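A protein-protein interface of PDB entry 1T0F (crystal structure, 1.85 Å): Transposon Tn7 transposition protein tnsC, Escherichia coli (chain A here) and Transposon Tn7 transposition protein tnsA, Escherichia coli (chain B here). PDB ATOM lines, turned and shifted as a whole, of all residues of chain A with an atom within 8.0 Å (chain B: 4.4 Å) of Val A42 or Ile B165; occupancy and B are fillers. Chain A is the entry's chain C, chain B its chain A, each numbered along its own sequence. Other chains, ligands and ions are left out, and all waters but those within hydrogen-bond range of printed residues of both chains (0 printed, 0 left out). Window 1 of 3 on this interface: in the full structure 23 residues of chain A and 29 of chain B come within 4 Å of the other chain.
Printed residues of chain B that touch a printed residue of chain A: Leu B149, Phe B164, Ile B165, Phe B166 and Thr B167.
Hydrophobic or aromatic side chains of chain B within 4 Å of the printed part of chain A: Leu B149, Phe B164, Ile B165 and Phe B166.
Of the 16 printed residues of chain A, 8 touch a printed residue of chain B.
Hydrophobic or aromatic side chains of chain A within 4 Å of the printed part of chain B: Leu A20, His A34, Val A42, Ile A43, Val A44 and Leu A49.
Among the printed residues, no Asp or Glu carboxylate lies within 4 Å of a Lys or Arg side-chain nitrogen of the other chain.
The backbone NH (N) of Gln B133 sits at hydrogen-bond distance from the backbone carbonyl oxygen (O) of Phe B164, 3.0 Å away.
The backbone carbonyl oxygen (O) of Gln B133 lies within hydrogen-bond range of the backbone NH (N) of Phe B166 (2.9 Å).
O of Leu A37 sits at hydrogen-bond distance from N of Val A42, at 3.0 Å.
O of Leu A37 lies within hydrogen-bond range of N of Ile A43 (3.3 Å).
Val A42 touches two residues of chain B.
Ile B165 touches just these residues of chain A: Val A42 (3.0 Å), Ile A43 (3.3 Å) and Val A44 (3.7 Å).
Printed residues of chain B within 4 Å of Asp A45: Phe B166 (3.4 Å).
Of the printed residues of chain B, His A34 touches Thr B167.
Of the printed residues of chain A, Phe B166 touches Val A44 (3.1 Å), Asp A45 (3.4 Å) and Leu A49 (3.8 Å).
Met A33 touches none of the printed residues of chain B.
Lys A40 touches none of the printed residues of chain B.
The nearest residue of chain A that does not touch Ile B165 is Leu A37 (4.2 Å).
Leu A20 touches Leu B149 (CD1 to CB, 3.7 Å).
His A34 touches Thr B167 (CD2 to OG1, 3.4 Å).
Phe B164 touches Gly A41.
Val A42 touches Phe B164 (O to CA, 3.4 Å).
CA of Ile A43 touches O of Ile B165 (3.3 Å).
Val A44 touches Phe B164.
O of Ile B165 touches N of Val A44 (3.7 Å).
Val A44 touches Phe B166.
C of Asp A45 touches CZ of Phe B166 (3.4 Å).
CD1 of Leu A49 touches CE1 of Phe B166 (3.8 Å).
The backbone NH (N) of Ile B165 is in hydrogen-bond range of the backbone carbonyl oxygen (O) of Val A42 (3.0 Å).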
ATOM      1  N   THR A  18      19.647  26.200  33.414  1.00  0.00           N
ATOM      2  CA  THR A  18      19.143  25.417  32.290  1.00  0.00           C
ATOM      3  C   THR A  18      20.173  25.130  31.209  1.00  0.00           C
ATOM      4  O   THR A  18      19.874  24.439  30.233  1.00  0.00           O
ATOM      5  CB  THR A  18      17.942  26.114  31.649  1.00  0.00           C
ATOM      6  OG1 THR A  18      18.320  27.431  31.244  1.00  0.00           O
ATOM      7  CG2 THR A  18      16.802  26.217  32.648  1.00  0.00           C
ATOM      8  N   LEU A  20      22.999  23.263  29.496  1.00  0.00           N
ATOM      9  CA  LEU A  20      23.421  21.874  29.536  1.00  0.00           C
ATOM     10  C   LEU A  20      24.809  21.705  30.145  1.00  0.00           C
ATOM     11  O   LEU A  20      25.098  20.685  30.771  1.00  0.00           O
ATOM     12  CB  LEU A  20      23.385  21.268  28.133  1.00  0.00           C
ATOM     13  CG  LEU A  20      21.991  21.237  27.486  1.00  0.00           C
ATOM     14  CD1 LEU A  20      22.071  20.548  26.135  1.00  0.00           C
ATOM     15  CD2 LEU A  20      21.006  20.514  28.399  1.00  0.00           C
ATOM     16  N   ILE A  23      24.404  21.865  33.940  1.00  0.00           N
ATOM     17  CA  ILE A  23      23.795  20.613  34.375  1.00  0.00           C
ATOM     18  C   ILE A  23      24.839  19.504  34.449  1.00  0.00           C
ATOM     19  O   ILE A  23      24.870  18.728  35.403  1.00  0.00           O
ATOM     20  CB  ILE A  23      22.652  20.215  33.427  1.00  0.00           C
ATOM     21  CG1 ILE A  23      21.505  21.221  33.579  1.00  0.00           C
ATOM     22  CG2 ILE A  23      22.194  18.785  33.715  1.00  0.00           C
ATOM     23  CD1 ILE A  23      20.439  21.125  32.483  1.00  0.00           C
ATOM     24  N   MET A  33      24.853  11.260  32.128  1.00  0.00           N
ATOM     25  CA  MET A  33      24.256  12.533  31.743  1.00  0.00           C
ATOM     26  C   MET A  33      22.875  12.191  31.188  1.00  0.00           C
ATOM     27  O   MET A  33      21.914  12.946  31.356  1.00  0.00           O
ATOM     28  CB  MET A  33      25.086  13.229  30.656  1.00  0.00           C
ATOM     29  CG  MET A  33      25.702  14.547  31.096  1.00  0.00           C
ATOM     30  SD  MET A  33      24.536  15.696  31.860  1.00  0.00           S
ATOM     31  CE  MET A  33      24.504  17.067  30.698  1.00  0.00           C
ATOM     32  N   HIS A  34      22.783  11.045  30.522  1.00  0.00           N
ATOM     33  CA  HIS A  34      21.507  10.621  29.970  1.00  0.00           C
ATOM     34  C   HIS A  34      20.468  10.562  31.086  1.00  0.00           C
ATOM     35  O   HIS A  34      19.384  11.142  30.980  1.00  0.00           O
ATOM     36  CB  HIS A  34      21.631   9.253  29.294  1.00  0.00           C
ATOM     37  CG  HIS A  34      20.310   8.639  28.954  1.00  0.00           C
ATOM     38  ND1 HIS A  34      19.572   7.920  29.869  1.00  0.00           N
ATOM     39  CD2 HIS A  34      19.552   8.715  27.836  1.00  0.00           C
ATOM     40  CE1 HIS A  34      18.414   7.583  29.329  1.00  0.00           C
ATOM     41  NE2 HIS A  34      18.375   8.054  28.096  1.00  0.00           N
ATOM     42  N   ARG A  36      20.435  12.015  33.948  1.00  0.00           N
ATOM     43  CA  ARG A  36      20.183  13.354  34.451  1.00  0.00           C
ATOM     44  C   ARG A  36      19.259  14.164  33.539  1.00  0.00           C
ATOM     45  O   ARG A  36      18.309  14.786  34.007  1.00  0.00           O
ATOM     46  CB  ARG A  36      21.516  14.089  34.631  1.00  0.00           C
ATOM     47  CG  ARG A  36      21.393  15.528  35.098  1.00  0.00           C
ATOM     48  CD  ARG A  36      20.579  15.644  36.371  1.00  0.00           C
ATOM     49  NE  ARG A  36      20.594  17.015  36.871  1.00  0.00           N
ATOM     50  CZ  ARG A  36      19.679  17.531  37.687  1.00  0.00           C
ATOM     51  NH1 ARG A  36      18.659  16.790  38.102  1.00  0.00           N
ATOM     52  NH2 ARG A  36      19.786  18.791  38.086  1.00  0.00           N
ATOM     53  N   LEU A  37      19.531  14.152  32.236  1.00  0.00           N
ATOM     54  CA  LEU A  37      18.713  14.912  31.299  1.00  0.00           C
ATOM     55  C   LEU A  37      17.313  14.329  31.138  1.00  0.00           C
ATOM     56  O   LEU A  37      16.359  15.073  30.916  1.00  0.00           O
ATOM     57  CB  LEU A  37      19.405  15.014  29.928  1.00  0.00           C
ATOM     58  CG  LEU A  37      20.672  15.880  29.884  1.00  0.00           C
ATOM     59  CD1 LEU A  37      21.262  15.873  28.471  1.00  0.00           C
ATOM     60  CD2 LEU A  37      20.347  17.308  30.322  1.00  0.00           C
ATOM     61  N   LYS A  38      17.182  13.009  31.258  1.00  0.00           N
ATOM     62  CA  LYS A  38      15.865  12.398  31.126  1.00  0.00           C
ATOM     63  C   LYS A  38      15.042  12.805  32.344  1.00  0.00           C
ATOM     64  O   LYS A  38      13.851  13.074  32.235  1.00  0.00           O
ATOM     65  CB  LYS A  38      15.965  10.872  31.022  1.00  0.00           C
ATOM     66  CG  LYS A  38      14.662  10.211  30.563  1.00  0.00           C
ATOM     67  CD  LYS A  38      14.906   8.838  29.953  1.00  0.00           C
ATOM     68  CE  LYS A  38      13.611   8.215  29.407  1.00  0.00           C
ATOM     69  NZ  LYS A  38      13.889   7.038  28.513  1.00  0.00           N
ATOM     70  N   GLY A  39      15.686  12.867  33.502  1.00  0.00           N
ATOM     71  CA  GLY A  39      14.975  13.266  34.701  1.00  0.00           C
ATOM     72  C   GLY A  39      14.434  14.681  34.601  1.00  0.00           C
ATOM     73  O   GLY A  39      13.383  14.996  35.167  1.00  0.00           O
ATOM     74  N   LYS A  40      15.146  15.540  33.872  1.00  0.00           N
ATOM     75  CA  LYS A  40      14.736  16.930  33.709  1.00  0.00           C
ATOM     76  C   LYS A  40      13.770  17.171  32.546  1.00  0.00           C
ATOM     77  O   LYS A  40      13.295  18.293  32.352  1.00  0.00           O
ATOM     78  CB  LYS A  40      15.963  17.830  33.533  1.00  0.00           C
ATOM     79  CG  LYS A  40      16.877  17.880  34.748  1.00  0.00           C
ATOM     80  CD  LYS A  40      17.692  19.168  34.781  1.00  0.00           C
ATOM     81  CE  LYS A  40      16.779  20.370  35.022  1.00  0.00           C
ATOM     82  NZ  LYS A  40      17.480  21.688  34.979  1.00  0.00           N
ATOM     83  N   GLY A  41      13.484  16.127  31.774  1.00  0.00           N
ATOM     84  CA  GLY A  41      12.574  16.287  30.657  1.00  0.00           C
ATOM     85  C   GLY A  41      13.234  16.814  29.392  1.00  0.00           C
ATOM     86  O   GLY A  41      12.546  17.169  28.432  1.00  0.00           O
ATOM     87  N   VAL A  42      14.561  16.889  29.387  1.00  0.00           N
ATOM     88  CA  VAL A  42      15.276  17.347  28.196  1.00  0.00           C
ATOM     89  C   VAL A  42      15.265  16.175  27.220  1.00  0.00           C
ATOM     90  O   VAL A  42      15.181  16.345  26.002  1.00  0.00           O
ATOM     91  CB  VAL A  42      16.733  17.738  28.528  1.00  0.00           C
ATOM     92  CG1 VAL A  42      17.491  18.044  27.243  1.00  0.00           C
ATOM     93  CG2 VAL A  42      16.744  18.955  29.443  1.00  0.00           C
ATOM     94  N   ILE A  43      15.368  14.972  27.775  1.00  0.00           N
ATOM     95  CA  ILE A  43      15.324  13.753  26.984  1.00  0.00           C
ATOM     96  C   ILE A  43      13.953  13.144  27.264  1.00  0.00           C
ATOM     97  O   ILE A  43      13.541  13.065  28.416  1.00  0.00           O
ATOM     98  CB  ILE A  43      16.407  12.750  27.423  1.00  0.00           C
ATOM     99  CG1 ILE A  43      17.796  13.282  27.042  1.00  0.00           C
ATOM    100  CG2 ILE A  43      16.168  11.389  26.762  1.00  0.00           C
ATOM    101  CD1 ILE A  43      18.933  12.400  27.499  1.00  0.00           C
ATOM    102  N   VAL A  44      13.241  12.744  26.215  1.00  0.00           N
ATOM    103  CA  VAL A  44      11.926  12.132  26.392  1.00  0.00           C
ATOM    104  C   VAL A  44      11.754  10.997  25.389  1.00  0.00           C
ATOM    105  O   VAL A  44      12.464  10.934  24.390  1.00  0.00           O
ATOM    106  CB  VAL A  44      10.776  13.154  26.149  1.00  0.00           C
ATOM    107  CG1 VAL A  44      10.891  14.333  27.109  1.00  0.00           C
ATOM    108  CG2 VAL A  44      10.807  13.634  24.707  1.00  0.00           C
ATOM    109  N   ASP A  45      10.827  10.088  25.657  1.00  0.00           N
ATOM    110  CA  ASP A  45      10.573   9.019  24.697  1.00  0.00           C
ATOM    111  C   ASP A  45       9.357   9.454  23.891  1.00  0.00           C
ATOM    112  O   ASP A  45       8.572  10.293  24.339  1.00  0.00           O
ATOM    113  CB  ASP A  45      10.323   7.672  25.389  1.00  0.00           C
ATOM    114  CG  ASP A  45       9.325   7.765  26.514  1.00  0.00           C
ATOM    115  OD1 ASP A  45       8.224   8.309  26.289  1.00  0.00           O
ATOM    116  OD2 ASP A  45       9.641   7.287  27.626  1.00  0.00           O
ATOM    117  N   LEU A  49       5.452  12.695  23.808  1.00  0.00           N
ATOM    118  CA  LEU A  49       5.156  13.759  22.852  1.00  0.00           C
ATOM    119  C   LEU A  49       3.827  13.617  22.123  1.00  0.00           C
ATOM    120  O   LEU A  49       3.404  14.539  21.420  1.00  0.00           O
ATOM    121  CB  LEU A  49       6.267  13.848  21.815  1.00  0.00           C
ATOM    122  CG  LEU A  49       7.679  14.053  22.352  1.00  0.00           C
ATOM    123  CD1 LEU A  49       8.658  13.999  21.190  1.00  0.00           C
ATOM    124  CD2 LEU A  49       7.763  15.379  23.090  1.00  0.00           C
ATOM    125  N   GLN B 133      16.896  16.350  18.426  1.00  0.00           N
ATOM    126  CA  GLN B 133      18.286  16.084  18.074  1.00  0.00           C
ATOM    127  C   GLN B 133      18.501  14.658  18.604  1.00  0.00           C
ATOM    128  O   GLN B 133      18.159  14.350  19.750  1.00  0.00           O
ATOM    129  CB  GLN B 133      19.261  17.051  18.766  1.00  0.00           C
ATOM    130  CG  GLN B 133      20.737  16.681  18.532  1.00  0.00           C
ATOM    131  CD  GLN B 133      21.185  16.817  17.080  1.00  0.00           C
ATOM    132  OE1 GLN B 133      22.123  16.143  16.641  1.00  0.00           O
ATOM    133  NE2 GLN B 133      20.534  17.700  16.336  1.00  0.00           N
ATOM    134  N   LEU B 149      25.125  20.980  21.678  1.00  0.00           N
ATOM    135  CA  LEU B 149      23.732  20.762  22.050  1.00  0.00           C
ATOM    136  C   LEU B 149      23.202  22.014  22.743  1.00  0.00           C
ATOM    137  O   LEU B 149      22.042  22.373  22.568  1.00  0.00           O
ATOM    138  CB  LEU B 149      23.607  19.548  22.972  1.00  0.00           C
ATOM    139  CG  LEU B 149      23.788  18.179  22.316  1.00  0.00           C
ATOM    140  CD1 LEU B 149      23.859  17.094  23.398  1.00  0.00           C
ATOM    141  CD2 LEU B 149      22.619  17.906  21.355  1.00  0.00           C
ATOM    142  N   TRP B 163      12.186  21.659  22.167  1.00  0.00           N
ATOM    143  CA  TRP B 163      13.300  20.888  21.619  1.00  0.00           C
ATOM    144  C   TRP B 163      13.673  19.801  22.610  1.00  0.00           C
ATOM    145  O   TRP B 163      13.734  20.059  23.818  1.00  0.00           O
ATOM    146  CB  TRP B 163      14.502  21.811  21.395  1.00  0.00           C
ATOM    147  CG  TRP B 163      15.753  21.114  20.968  1.00  0.00           C
ATOM    148  CD1 TRP B 163      16.081  20.710  19.708  1.00  0.00           C
ATOM    149  CD2 TRP B 163      16.871  20.786  21.800  1.00  0.00           C
ATOM    150  NE1 TRP B 163      17.342  20.156  19.700  1.00  0.00           N
ATOM    151  CE2 TRP B 163      17.847  20.190  20.974  1.00  0.00           C
ATOM    152  CE3 TRP B 163      17.140  20.937  23.167  1.00  0.00           C
ATOM    153  CZ2 TRP B 163      19.078  19.750  21.470  1.00  0.00           C
ATOM    154  CZ3 TRP B 163      18.366  20.496  23.661  1.00  0.00           C
ATOM    155  CH2 TRP B 163      19.316  19.911  22.813  1.00  0.00           C
ATOM    156  N   PHE B 164      13.928  18.598  22.097  1.00  0.00           N
ATOM    157  CA  PHE B 164      14.286  17.450  22.922  1.00  0.00           C
ATOM    158  C   PHE B 164      15.418  16.649  22.311  1.00  0.00           C
ATOM    159  O   PHE B 164      15.665  16.702  21.102  1.00  0.00           O
ATOM    160  CB  PHE B 164      13.094  16.495  23.057  1.00  0.00           C
ATOM    161  CG  PHE B 164      11.853  17.147  23.561  1.00  0.00           C
ATOM    162  CD1 PHE B 164      11.634  17.289  24.926  1.00  0.00           C
ATOM    163  CD2 PHE B 164      10.911  17.653  22.668  1.00  0.00           C
ATOM    164  CE1 PHE B 164      10.494  17.931  25.399  1.00  0.00           C
ATOM    165  CE2 PHE B 164       9.766  18.300  23.126  1.00  0.00           C
ATOM    166  CZ  PHE B 164       9.556  18.439  24.493  1.00  0.00           C
ATOM    167  N   ILE B 165      16.082  15.877  23.157  1.00  0.00           N
ATOM    168  CA  ILE B 165      17.140  14.994  22.714  1.00  0.00           C
ATOM    169  C   ILE B 165      16.595  13.566  22.805  1.00  0.00           C
ATOM    170  O   ILE B 165      15.917  13.220  23.762  1.00  0.00           O
ATOM    171  CB  ILE B 165      18.378  15.105  23.618  1.00  0.00           C
ATOM    172  CG1 ILE B 165      19.005  16.492  23.463  1.00  0.00           C
ATOM    173  CG2 ILE B 165      19.372  14.003  23.270  1.00  0.00           C
ATOM    174  CD1 ILE B 165      20.024  16.802  24.537  1.00  0.00           C
ATOM    175  N   PHE B 166      16.874  12.761  21.791  1.00  0.00           N
ATOM    176  CA  PHE B 166      16.448  11.363  21.758  1.00  0.00           C
ATOM    177  C   PHE B 166      17.686  10.494  21.612  1.00  0.00           C
ATOM    178  O   PHE B 166      18.527  10.761  20.756  1.00  0.00           O
ATOM    179  CB  PHE B 166      15.537  11.094  20.551  1.00  0.00           C
ATOM    180  CG  PHE B 166      14.077  11.021  20.888  1.00  0.00           C
ATOM    181  CD1 PHE B 166      13.321  12.183  21.034  1.00  0.00           C
ATOM    182  CD2 PHE B 166      13.458   9.787  21.067  1.00  0.00           C
ATOM    183  CE1 PHE B 166      11.956  12.115  21.355  1.00  0.00           C
ATOM    184  CE2 PHE B 166      12.107   9.703  21.388  1.00  0.00           C
ATOM    185  CZ  PHE B 166      11.351  10.872  21.533  1.00  0.00           C
ATOM    186  N   THR B 167      17.807   9.454  22.435  1.00  0.00           N
ATOM    187  CA  THR B 167      18.955   8.552  22.326  1.00  0.00           C
ATOM    188  C   THR B 167      18.463   7.129  22.075  1.00  0.00           C
ATOM    189  O   THR B 167      17.256   6.875  22.028  1.00  0.00           O
ATOM    190  CB  THR B 167      19.820   8.525  23.616  1.00  0.00           C
ATOM    191  OG1 THR B 167      19.158   7.753  24.623  1.00  0.00           O
ATOM    192  CG2 THR B 167      20.065   9.937  24.141  1.00  0.00           C
